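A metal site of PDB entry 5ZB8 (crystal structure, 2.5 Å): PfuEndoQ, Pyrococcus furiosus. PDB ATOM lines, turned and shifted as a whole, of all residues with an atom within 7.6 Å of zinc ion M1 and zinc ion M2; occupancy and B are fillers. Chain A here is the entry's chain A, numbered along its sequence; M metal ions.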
ATOM      1  N   HIS A   8      -7.846   7.140  15.133  1.00  0.00           N
ATOM      2  CA  HIS A   8      -7.355   8.236  14.300  1.00  0.00           C
ATOM      3  C   HIS A   8      -8.342   8.477  13.178  1.00  0.00           C
ATOM      4  O   HIS A   8      -8.415   7.702  12.228  1.00  0.00           O
ATOM      5  CB  HIS A   8      -5.955   7.931  13.756  1.00  0.00           C
ATOM      6  CG  HIS A   8      -5.351   9.053  12.958  1.00  0.00           C
ATOM      7  ND1 HIS A   8      -4.094   8.967  12.407  1.00  0.00           N
ATOM      8  CD2 HIS A   8      -5.820  10.282  12.645  1.00  0.00           C
ATOM      9  CE1 HIS A   8      -3.819  10.097  11.767  1.00  0.00           C
ATOM     10  NE2 HIS A   8      -4.853  10.907  11.893  1.00  0.00           N
ATOM     11  N   ILE A   9      -9.128   9.554  13.297  1.00  0.00           N
ATOM     12  CA  ILE A   9     -10.025  10.030  12.259  1.00  0.00           C
ATOM     13  C   ILE A   9      -9.911  11.548  12.194  1.00  0.00           C
ATOM     14  O   ILE A   9      -9.130  12.162  12.928  1.00  0.00           O
ATOM     15  CB  ILE A   9     -11.486   9.611  12.494  1.00  0.00           C
ATOM     16  CG1 ILE A   9     -12.056  10.296  13.734  1.00  0.00           C
ATOM     17  CG2 ILE A   9     -11.603   8.097  12.623  1.00  0.00           C
ATOM     18  CD1 ILE A   9     -13.522  10.019  13.972  1.00  0.00           C
ATOM     19  N   HIS A  10     -10.699  12.160  11.322  1.00  0.00           N
ATOM     20  CA  HIS A  10     -10.715  13.607  11.181  1.00  0.00           C
ATOM     21  C   HIS A  10     -12.150  14.089  11.063  1.00  0.00           C
ATOM     22  O   HIS A  10     -13.023  13.393  10.540  1.00  0.00           O
ATOM     23  CB  HIS A  10      -9.891  14.079   9.975  1.00  0.00           C
ATOM     24  CG  HIS A  10      -8.416  13.939  10.171  1.00  0.00           C
ATOM     25  ND1 HIS A  10      -7.683  14.801  10.958  1.00  0.00           N
ATOM     26  CD2 HIS A  10      -7.534  13.036   9.686  1.00  0.00           C
ATOM     27  CE1 HIS A  10      -6.420  14.438  10.944  1.00  0.00           C
ATOM     28  NE2 HIS A  10      -6.301  13.366  10.185  1.00  0.00           N
ATOM     29  N   SER A  14     -11.352  19.553   9.262  1.00  0.00           N
ATOM     30  CA  SER A  14     -10.052  19.304   8.660  1.00  0.00           C
ATOM     31  C   SER A  14     -10.093  19.534   7.149  1.00  0.00           C
ATOM     32  O   SER A  14     -11.147  19.413   6.515  1.00  0.00           O
ATOM     33  CB  SER A  14      -9.571  17.884   8.947  1.00  0.00           C
ATOM     34  OG  SER A  14      -9.136  17.738  10.286  1.00  0.00           O
ATOM     35  N   ASP A  42      -9.216  15.604  15.964  1.00  0.00           N
ATOM     36  CA  ASP A  42      -9.326  17.074  15.921  1.00  0.00           C
ATOM     37  C   ASP A  42      -9.692  17.676  17.276  1.00  0.00           C
ATOM     38  O   ASP A  42     -10.355  18.713  17.342  1.00  0.00           O
ATOM     39  CB  ASP A  42     -10.341  17.508  14.862  1.00  0.00           C
ATOM     40  CG  ASP A  42      -9.973  17.044  13.474  1.00  0.00           C
ATOM     41  OD1 ASP A  42      -9.009  16.265  13.329  1.00  0.00           O
ATOM     42  OD2 ASP A  42     -10.662  17.454  12.521  1.00  0.00           O
ATOM     43  N   CYS A  75      -6.201  13.499  18.726  1.00  0.00           N
ATOM     44  CA  CYS A  75      -5.914  14.584  17.798  1.00  0.00           C
ATOM     45  C   CYS A  75      -4.597  14.285  17.093  1.00  0.00           C
ATOM     46  O   CYS A  75      -3.743  13.555  17.598  1.00  0.00           O
ATOM     47  CB  CYS A  75      -5.845  15.935  18.508  1.00  0.00           C
ATOM     48  SG  CYS A  75      -5.693  17.349  17.389  1.00  0.00           S
ATOM     49  N   GLU A  76      -4.437  14.868  15.904  1.00  0.00           N
ATOM     50  CA  GLU A  76      -3.235  14.739  15.103  1.00  0.00           C
ATOM     51  C   GLU A  76      -2.674  16.115  14.807  1.00  0.00           C
ATOM     52  O   GLU A  76      -3.414  17.012  14.396  1.00  0.00           O
ATOM     53  CB  GLU A  76      -3.523  13.990  13.789  1.00  0.00           C
ATOM     54  CG  GLU A  76      -2.274  13.610  13.006  1.00  0.00           C
ATOM     55  CD  GLU A  76      -2.584  13.184  11.578  1.00  0.00           C
ATOM     56  OE1 GLU A  76      -3.576  13.676  11.016  1.00  0.00           O
ATOM     57  OE2 GLU A  76      -1.828  12.355  11.018  1.00  0.00           O
ATOM     58  N   VAL A  77      -1.368  16.289  15.016  1.00  0.00           N
ATOM     59  CA  VAL A  77      -0.708  17.565  14.791  1.00  0.00           C
ATOM     60  C   VAL A  77       0.404  17.378  13.765  1.00  0.00           C
ATOM     61  O   VAL A  77       0.905  16.275  13.548  1.00  0.00           O
ATOM     62  CB  VAL A  77      -0.140  18.171  16.087  1.00  0.00           C
ATOM     63  CG1 VAL A  77      -1.257  18.430  17.086  1.00  0.00           C
ATOM     64  CG2 VAL A  77       0.907  17.242  16.693  1.00  0.00           C
ATOM     65  N   GLU A  78       0.787  18.490  13.146  1.00  0.00           N
ATOM     66  CA  GLU A  78       1.839  18.529  12.139  1.00  0.00           C
ATOM     67  C   GLU A  78       2.941  19.461  12.628  1.00  0.00           C
ATOM     68  O   GLU A  78       2.664  20.589  13.037  1.00  0.00           O
ATOM     69  CB  GLU A  78       1.283  18.991  10.785  1.00  0.00           C
ATOM     70  CG  GLU A  78       2.323  19.224   9.717  1.00  0.00           C
ATOM     71  CD  GLU A  78       1.728  19.372   8.328  1.00  0.00           C
ATOM     72  OE1 GLU A  78       0.958  18.474   7.917  1.00  0.00           O
ATOM     73  OE2 GLU A  78       2.009  20.396   7.664  1.00  0.00           O
ATOM     74  N   ARG A  82       6.615  18.923   8.800  1.00  0.00           N
ATOM     75  CA  ARG A  82       5.379  18.357   8.262  1.00  0.00           C
ATOM     76  C   ARG A  82       5.157  16.899   8.691  1.00  0.00           C
ATOM     77  O   ARG A  82       4.387  16.183   8.054  1.00  0.00           O
ATOM     78  CB  ARG A  82       5.316  18.468   6.739  1.00  0.00           C
ATOM     79  CG  ARG A  82       4.859  19.836   6.241  1.00  0.00           C
ATOM     80  CD  ARG A  82       4.511  19.801   4.760  1.00  0.00           C
ATOM     81  NE  ARG A  82       3.413  20.710   4.446  1.00  0.00           N
ATOM     82  CZ  ARG A  82       2.140  20.328   4.365  1.00  0.00           C
ATOM     83  NH1 ARG A  82       1.804  19.054   4.562  1.00  0.00           N
ATOM     84  NH2 ARG A  82       1.192  21.220   4.075  1.00  0.00           N
ATOM     85  N   VAL A  83       5.815  16.466   9.761  1.00  0.00           N
ATOM     86  CA  VAL A  83       5.616  15.117  10.281  1.00  0.00           C
ATOM     87  C   VAL A  83       4.382  15.087  11.163  1.00  0.00           C
ATOM     88  O   VAL A  83       4.157  15.993  11.976  1.00  0.00           O
ATOM     89  CB  VAL A  83       6.866  14.642  11.045  1.00  0.00           C
ATOM     90  CG1 VAL A  83       6.605  13.291  11.715  1.00  0.00           C
ATOM     91  CG2 VAL A  83       8.056  14.544  10.117  1.00  0.00           C
ATOM     92  N   HIS A  84       3.556  14.055  11.000  1.00  0.00           N
ATOM     93  CA  HIS A  84       2.311  13.927  11.739  1.00  0.00           C
ATOM     94  C   HIS A  84       2.493  13.079  12.986  1.00  0.00           C
ATOM     95  O   HIS A  84       3.142  12.031  12.957  1.00  0.00           O
ATOM     96  CB  HIS A  84       1.233  13.316  10.851  1.00  0.00           C
ATOM     97  CG  HIS A  84       0.713  14.241   9.792  1.00  0.00           C
ATOM     98  ND1 HIS A  84      -0.248  13.868   8.878  1.00  0.00           N
ATOM     99  CD2 HIS A  84       1.016  15.527   9.514  1.00  0.00           C
ATOM    100  CE1 HIS A  84      -0.515  14.878   8.079  1.00  0.00           C
ATOM    101  NE2 HIS A  84       0.244  15.905   8.437  1.00  0.00           N
ATOM    102  N   HIS A  85       1.903  13.550  14.083  1.00  0.00           N
ATOM    103  CA  HIS A  85       1.959  12.857  15.371  1.00  0.00           C
ATOM    104  C   HIS A  85       0.560  12.724  15.931  1.00  0.00           C
ATOM    105  O   HIS A  85      -0.233  13.656  15.870  1.00  0.00           O
ATOM    106  CB  HIS A  85       2.851  13.611  16.364  1.00  0.00           C
ATOM    107  CG  HIS A  85       4.203  13.965  15.828  1.00  0.00           C
ATOM    108  ND1 HIS A  85       5.303  13.149  15.971  1.00  0.00           N
ATOM    109  CD2 HIS A  85       4.632  15.066  15.153  1.00  0.00           C
ATOM    110  CE1 HIS A  85       6.355  13.725  15.406  1.00  0.00           C
ATOM    111  NE2 HIS A  85       5.976  14.884  14.902  1.00  0.00           N
ATOM    112  N   LEU A  86       0.271  11.552  16.486  1.00  0.00           N
ATOM    113  CA  LEU A  86      -1.043  11.239  17.054  1.00  0.00           C
ATOM    114  C   LEU A  86      -1.000  11.448  18.563  1.00  0.00           C
ATOM    115  O   LEU A  86      -0.064  11.000  19.233  1.00  0.00           O
ATOM    116  CB  LEU A  86      -1.461   9.812  16.717  1.00  0.00           C
ATOM    117  CG  LEU A  86      -2.782   9.297  17.268  1.00  0.00           C
ATOM    118  CD1 LEU A  86      -3.953  10.156  16.792  1.00  0.00           C
ATOM    119  CD2 LEU A  86      -2.996   7.843  16.882  1.00  0.00           C
ATOM    120  N   ARG A 114      -6.518  19.873  11.771  1.00  0.00           N
ATOM    121  CA  ARG A 114      -5.186  19.371  12.095  1.00  0.00           C
ATOM    122  C   ARG A 114      -4.236  20.555  12.244  1.00  0.00           C
ATOM    123  O   ARG A 114      -3.758  21.103  11.241  1.00  0.00           O
ATOM    124  CB  ARG A 114      -4.684  18.431  10.996  1.00  0.00           C
ATOM    125  CG  ARG A 114      -3.284  17.882  11.218  1.00  0.00           C
ATOM    126  CD  ARG A 114      -3.010  16.753  10.231  1.00  0.00           C
ATOM    127  NE  ARG A 114      -3.330  17.150   8.866  1.00  0.00           N
ATOM    128  CZ  ARG A 114      -3.718  16.305   7.914  1.00  0.00           C
ATOM    129  NH1 ARG A 114      -3.846  15.014   8.190  1.00  0.00           N
ATOM    130  NH2 ARG A 114      -3.995  16.747   6.701  1.00  0.00           N
ATOM    131  N   ALA A 138       2.250   9.250  13.697  1.00  0.00           N
ATOM    132  CA  ALA A 138       1.129   8.771  12.903  1.00  0.00           C
ATOM    133  C   ALA A 138       1.637   8.200  11.580  1.00  0.00           C
ATOM    134  O   ALA A 138       2.600   8.695  11.004  1.00  0.00           O
ATOM    135  CB  ALA A 138       0.138   9.906  12.629  1.00  0.00           C
ATOM    136  N   HIS A 139       0.952   7.140  11.119  1.00  0.00           N
ATOM    137  CA  HIS A 139       1.263   6.416   9.877  1.00  0.00           C
ATOM    138  C   HIS A 139       2.741   6.491   9.527  1.00  0.00           C
ATOM    139  O   HIS A 139       3.125   7.100   8.516  1.00  0.00           O
ATOM    140  CB  HIS A 139       0.410   6.962   8.720  1.00  0.00           C
ATOM    141  CG  HIS A 139       0.261   8.451   8.726  1.00  0.00           C
ATOM    142  ND1 HIS A 139       1.296   9.308   8.431  1.00  0.00           N
ATOM    143  CD2 HIS A 139      -0.810   9.235   8.999  1.00  0.00           C
ATOM    144  CE1 HIS A 139       0.873  10.559   8.512  1.00  0.00           C
ATOM    145  NE2 HIS A 139      -0.401  10.542   8.857  1.00  0.00           N
ATOM    146  N   THR A 142       4.172   5.906   5.879  1.00  0.00           N
ATOM    147  CA  THR A 142       3.543   6.507   4.708  1.00  0.00           C
ATOM    148  C   THR A 142       4.545   7.424   3.998  1.00  0.00           C
ATOM    149  O   THR A 142       5.346   8.095   4.651  1.00  0.00           O
ATOM    150  CB  THR A 142       2.298   7.290   5.139  1.00  0.00           C
ATOM    151  OG1 THR A 142       1.321   6.378   5.653  1.00  0.00           O
ATOM    152  CG2 THR A 142       1.680   8.064   3.983  1.00  0.00           C
ATOM    153  N   TRP A 144       4.522  10.257   2.908  1.00  0.00           N
ATOM    154  CA  TRP A 144       4.339  11.692   3.045  1.00  0.00           C
ATOM    155  C   TRP A 144       3.876  12.017   4.452  1.00  0.00           C
ATOM    156  O   TRP A 144       3.123  11.248   5.074  1.00  0.00           O
ATOM    157  CB  TRP A 144       3.330  12.234   2.023  1.00  0.00           C
ATOM    158  CG  TRP A 144       2.095  11.400   1.916  1.00  0.00           C
ATOM    159  CD1 TRP A 144       1.026  11.401   2.763  1.00  0.00           C
ATOM    160  CD2 TRP A 144       1.802  10.438   0.899  1.00  0.00           C
ATOM    161  NE1 TRP A 144       0.081  10.494   2.338  1.00  0.00           N
ATOM    162  CE2 TRP A 144       0.536   9.893   1.193  1.00  0.00           C
ATOM    163  CE3 TRP A 144       2.479   9.976  -0.230  1.00  0.00           C
ATOM    164  CZ2 TRP A 144      -0.062   8.910   0.401  1.00  0.00           C
ATOM    165  CZ3 TRP A 144       1.888   9.010  -1.023  1.00  0.00           C
ATOM    166  CH2 TRP A 144       0.630   8.493  -0.701  1.00  0.00           C
ATOM    167  N   THR A 145       4.336  13.164   4.957  1.00  0.00           N
ATOM    168  CA  THR A 145       3.949  13.685   6.278  1.00  0.00           C
ATOM    169  C   THR A 145       4.156  12.646   7.363  1.00  0.00           C
ATOM    170  O   THR A 145       3.357  12.512   8.293  1.00  0.00           O
ATOM    171  CB  THR A 145       2.497  14.174   6.276  1.00  0.00           C
ATOM    172  OG1 THR A 145       1.599  13.056   6.149  1.00  0.00           O
ATOM    173  CG2 THR A 145       2.255  15.131   5.116  1.00  0.00           C
ATOM    174  N   SER A 146       5.253  11.896   7.265  1.00  0.00           N
ATOM    175  CA  SER A 146       5.492  10.776   8.166  1.00  0.00           C
ATOM    176  C   SER A 146       6.919  10.795   8.692  1.00  0.00           C
ATOM    177  O   SER A 146       7.822  11.374   8.090  1.00  0.00           O
ATOM    178  CB  SER A 146       5.216   9.445   7.470  1.00  0.00           C
ATOM    179  OG  SER A 146       3.855   9.346   7.105  1.00  0.00           O
ATOM    180  N   GLU A 167       2.010   4.280  15.126  1.00  0.00           N
ATOM    181  CA  GLU A 167       0.905   3.974  14.225  1.00  0.00           C
ATOM    182  C   GLU A 167       1.474   3.471  12.909  1.00  0.00           C
ATOM    183  O   GLU A 167       2.279   4.163  12.264  1.00  0.00           O
ATOM    184  CB  GLU A 167       0.019   5.197  14.009  1.00  0.00           C
ATOM    185  CG  GLU A 167      -1.153   4.945  13.068  1.00  0.00           C
ATOM    186  CD  GLU A 167      -2.065   6.146  12.941  1.00  0.00           C
ATOM    187  OE1 GLU A 167      -2.920   6.348  13.827  1.00  0.00           O
ATOM    188  OE2 GLU A 167      -1.930   6.897  11.950  1.00  0.00           O
ATOM    189  N   SER A 192      -7.521   4.036  10.937  1.00  0.00           N
ATOM    190  CA  SER A 192      -7.959   4.226   9.557  1.00  0.00           C
ATOM    191  C   SER A 192      -7.519   5.562   8.976  1.00  0.00           C
ATOM    192  O   SER A 192      -7.325   5.658   7.754  1.00  0.00           O
ATOM    193  CB  SER A 192      -9.484   4.102   9.470  1.00  0.00           C
ATOM    194  OG  SER A 192     -10.119   5.232  10.040  1.00  0.00           O
ATOM    195  N   ASP A 193      -7.366   6.593   9.799  1.00  0.00           N
ATOM    196  CA  ASP A 193      -7.165   7.962   9.329  1.00  0.00           C
ATOM    197  C   ASP A 193      -8.321   8.374   8.409  1.00  0.00           C
ATOM    198  O   ASP A 193      -8.118   8.897   7.306  1.00  0.00           O
ATOM    199  CB  ASP A 193      -5.808   8.122   8.632  1.00  0.00           C
ATOM    200  CG  ASP A 193      -5.415   9.573   8.409  1.00  0.00           C
ATOM    201  OD1 ASP A 193      -6.105  10.466   8.941  1.00  0.00           O
ATOM    202  OD2 ASP A 193      -4.413   9.821   7.711  1.00  0.00           O
ATOM    203  N   ALA A 194      -9.535   8.111   8.878  1.00  0.00           N
ATOM    204  CA  ALA A 194     -10.721   8.234   8.037  1.00  0.00           C
ATOM    205  C   ALA A 194     -11.010   9.690   7.697  1.00  0.00           C
ATOM    206  O   ALA A 194     -11.035  10.558   8.583  1.00  0.00           O
ATOM    207  CB  ALA A 194     -11.921   7.606   8.728  1.00  0.00           C
ATOM    208  N   HIS A 195     -11.224   9.959   6.416  1.00  0.00           N
ATOM    209  CA  HIS A 195     -11.658  11.273   5.943  1.00  0.00           C
ATOM    210  C   HIS A 195     -13.127  11.299   5.552  1.00  0.00           C
ATOM    211  O   HIS A 195     -13.621  12.342   5.111  1.00  0.00           O
ATOM    212  CB  HIS A 195     -10.784  11.717   4.765  1.00  0.00           C
ATOM    213  CG  HIS A 195      -9.393  12.108   5.145  1.00  0.00           C
ATOM    214  ND1 HIS A 195      -8.622  11.371   6.025  1.00  0.00           N
ATOM    215  CD2 HIS A 195      -8.629  13.164   4.775  1.00  0.00           C
ATOM    216  CE1 HIS A 195      -7.450  11.962   6.179  1.00  0.00           C
ATOM    217  NE2 HIS A 195      -7.428  13.051   5.429  1.00  0.00           N
HETATM  218 ZN    ZN M   1      -4.652  12.037   9.957  1.00  0.00          ZN
HETATM  219 ZN    ZN M   2      -1.680  12.276   8.872  1.00  0.00          ZN
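Zinc ion M1 is bound by NE2 of His 10 (2.1 Å), OE1 of Glu 76 (2.2 Å), NE2 of His 8 (2.3 Å) and OD1 of Asp 193 (2.4 Å).
Merely in contact with zinc ion M2: Arg 114. Five residues have an atom within 4 Å of zinc ion M2: Glu 76, His 84, Arg 114, His 139 and Asp 193.
Zinc ion M2 is bound by ND1 of His 84 (2.1 Å), OE2 of Glu 76 (2.2 Å) and NE2 of His 139 (2.2 Å). Zinc ion M2 has three donor atoms within binding distance.
OG of Ser 146 sits at hydrogen-bond distance from O of His 139 (2.8 Å). ND1 of His 195 lies within hydrogen-bond range of O of Asp 193, at 2.8 Å. O of His 84 sits at hydrogen-bond distance from N of Ala 138 (3.0 Å). NE2 of His 84 lies within hydrogen-bond range of OE1 of Glu 78, at 2.7 Å. The side-chain carboxylate of Glu 167 sits at hydrogen-bond distance from a ring nitrogen (ND1) of His 8 (3.0 Å). The backbone NH (N) of His 10 lies within hydrogen-bond range of the backbone carbonyl oxygen (O) of Ala 194, 3.2 Å away. NH1 of Arg 114 sits close to OE1 of Glu 76. The side-chain hydroxyl (OG1) of Thr 142 lies close to the backbone carbonyl oxygen (O) of His 139 (3.5 Å).
Arg 114 touches zinc ion M1 (NH1 to ZN, 3.6 Å). Within 4 Å of zinc ion M1: His 8, His 10, Glu 76, Arg 114 and Asp 193. The nearest printed residue that does not touch zinc ion M1 is His 139 (4.6 Å).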
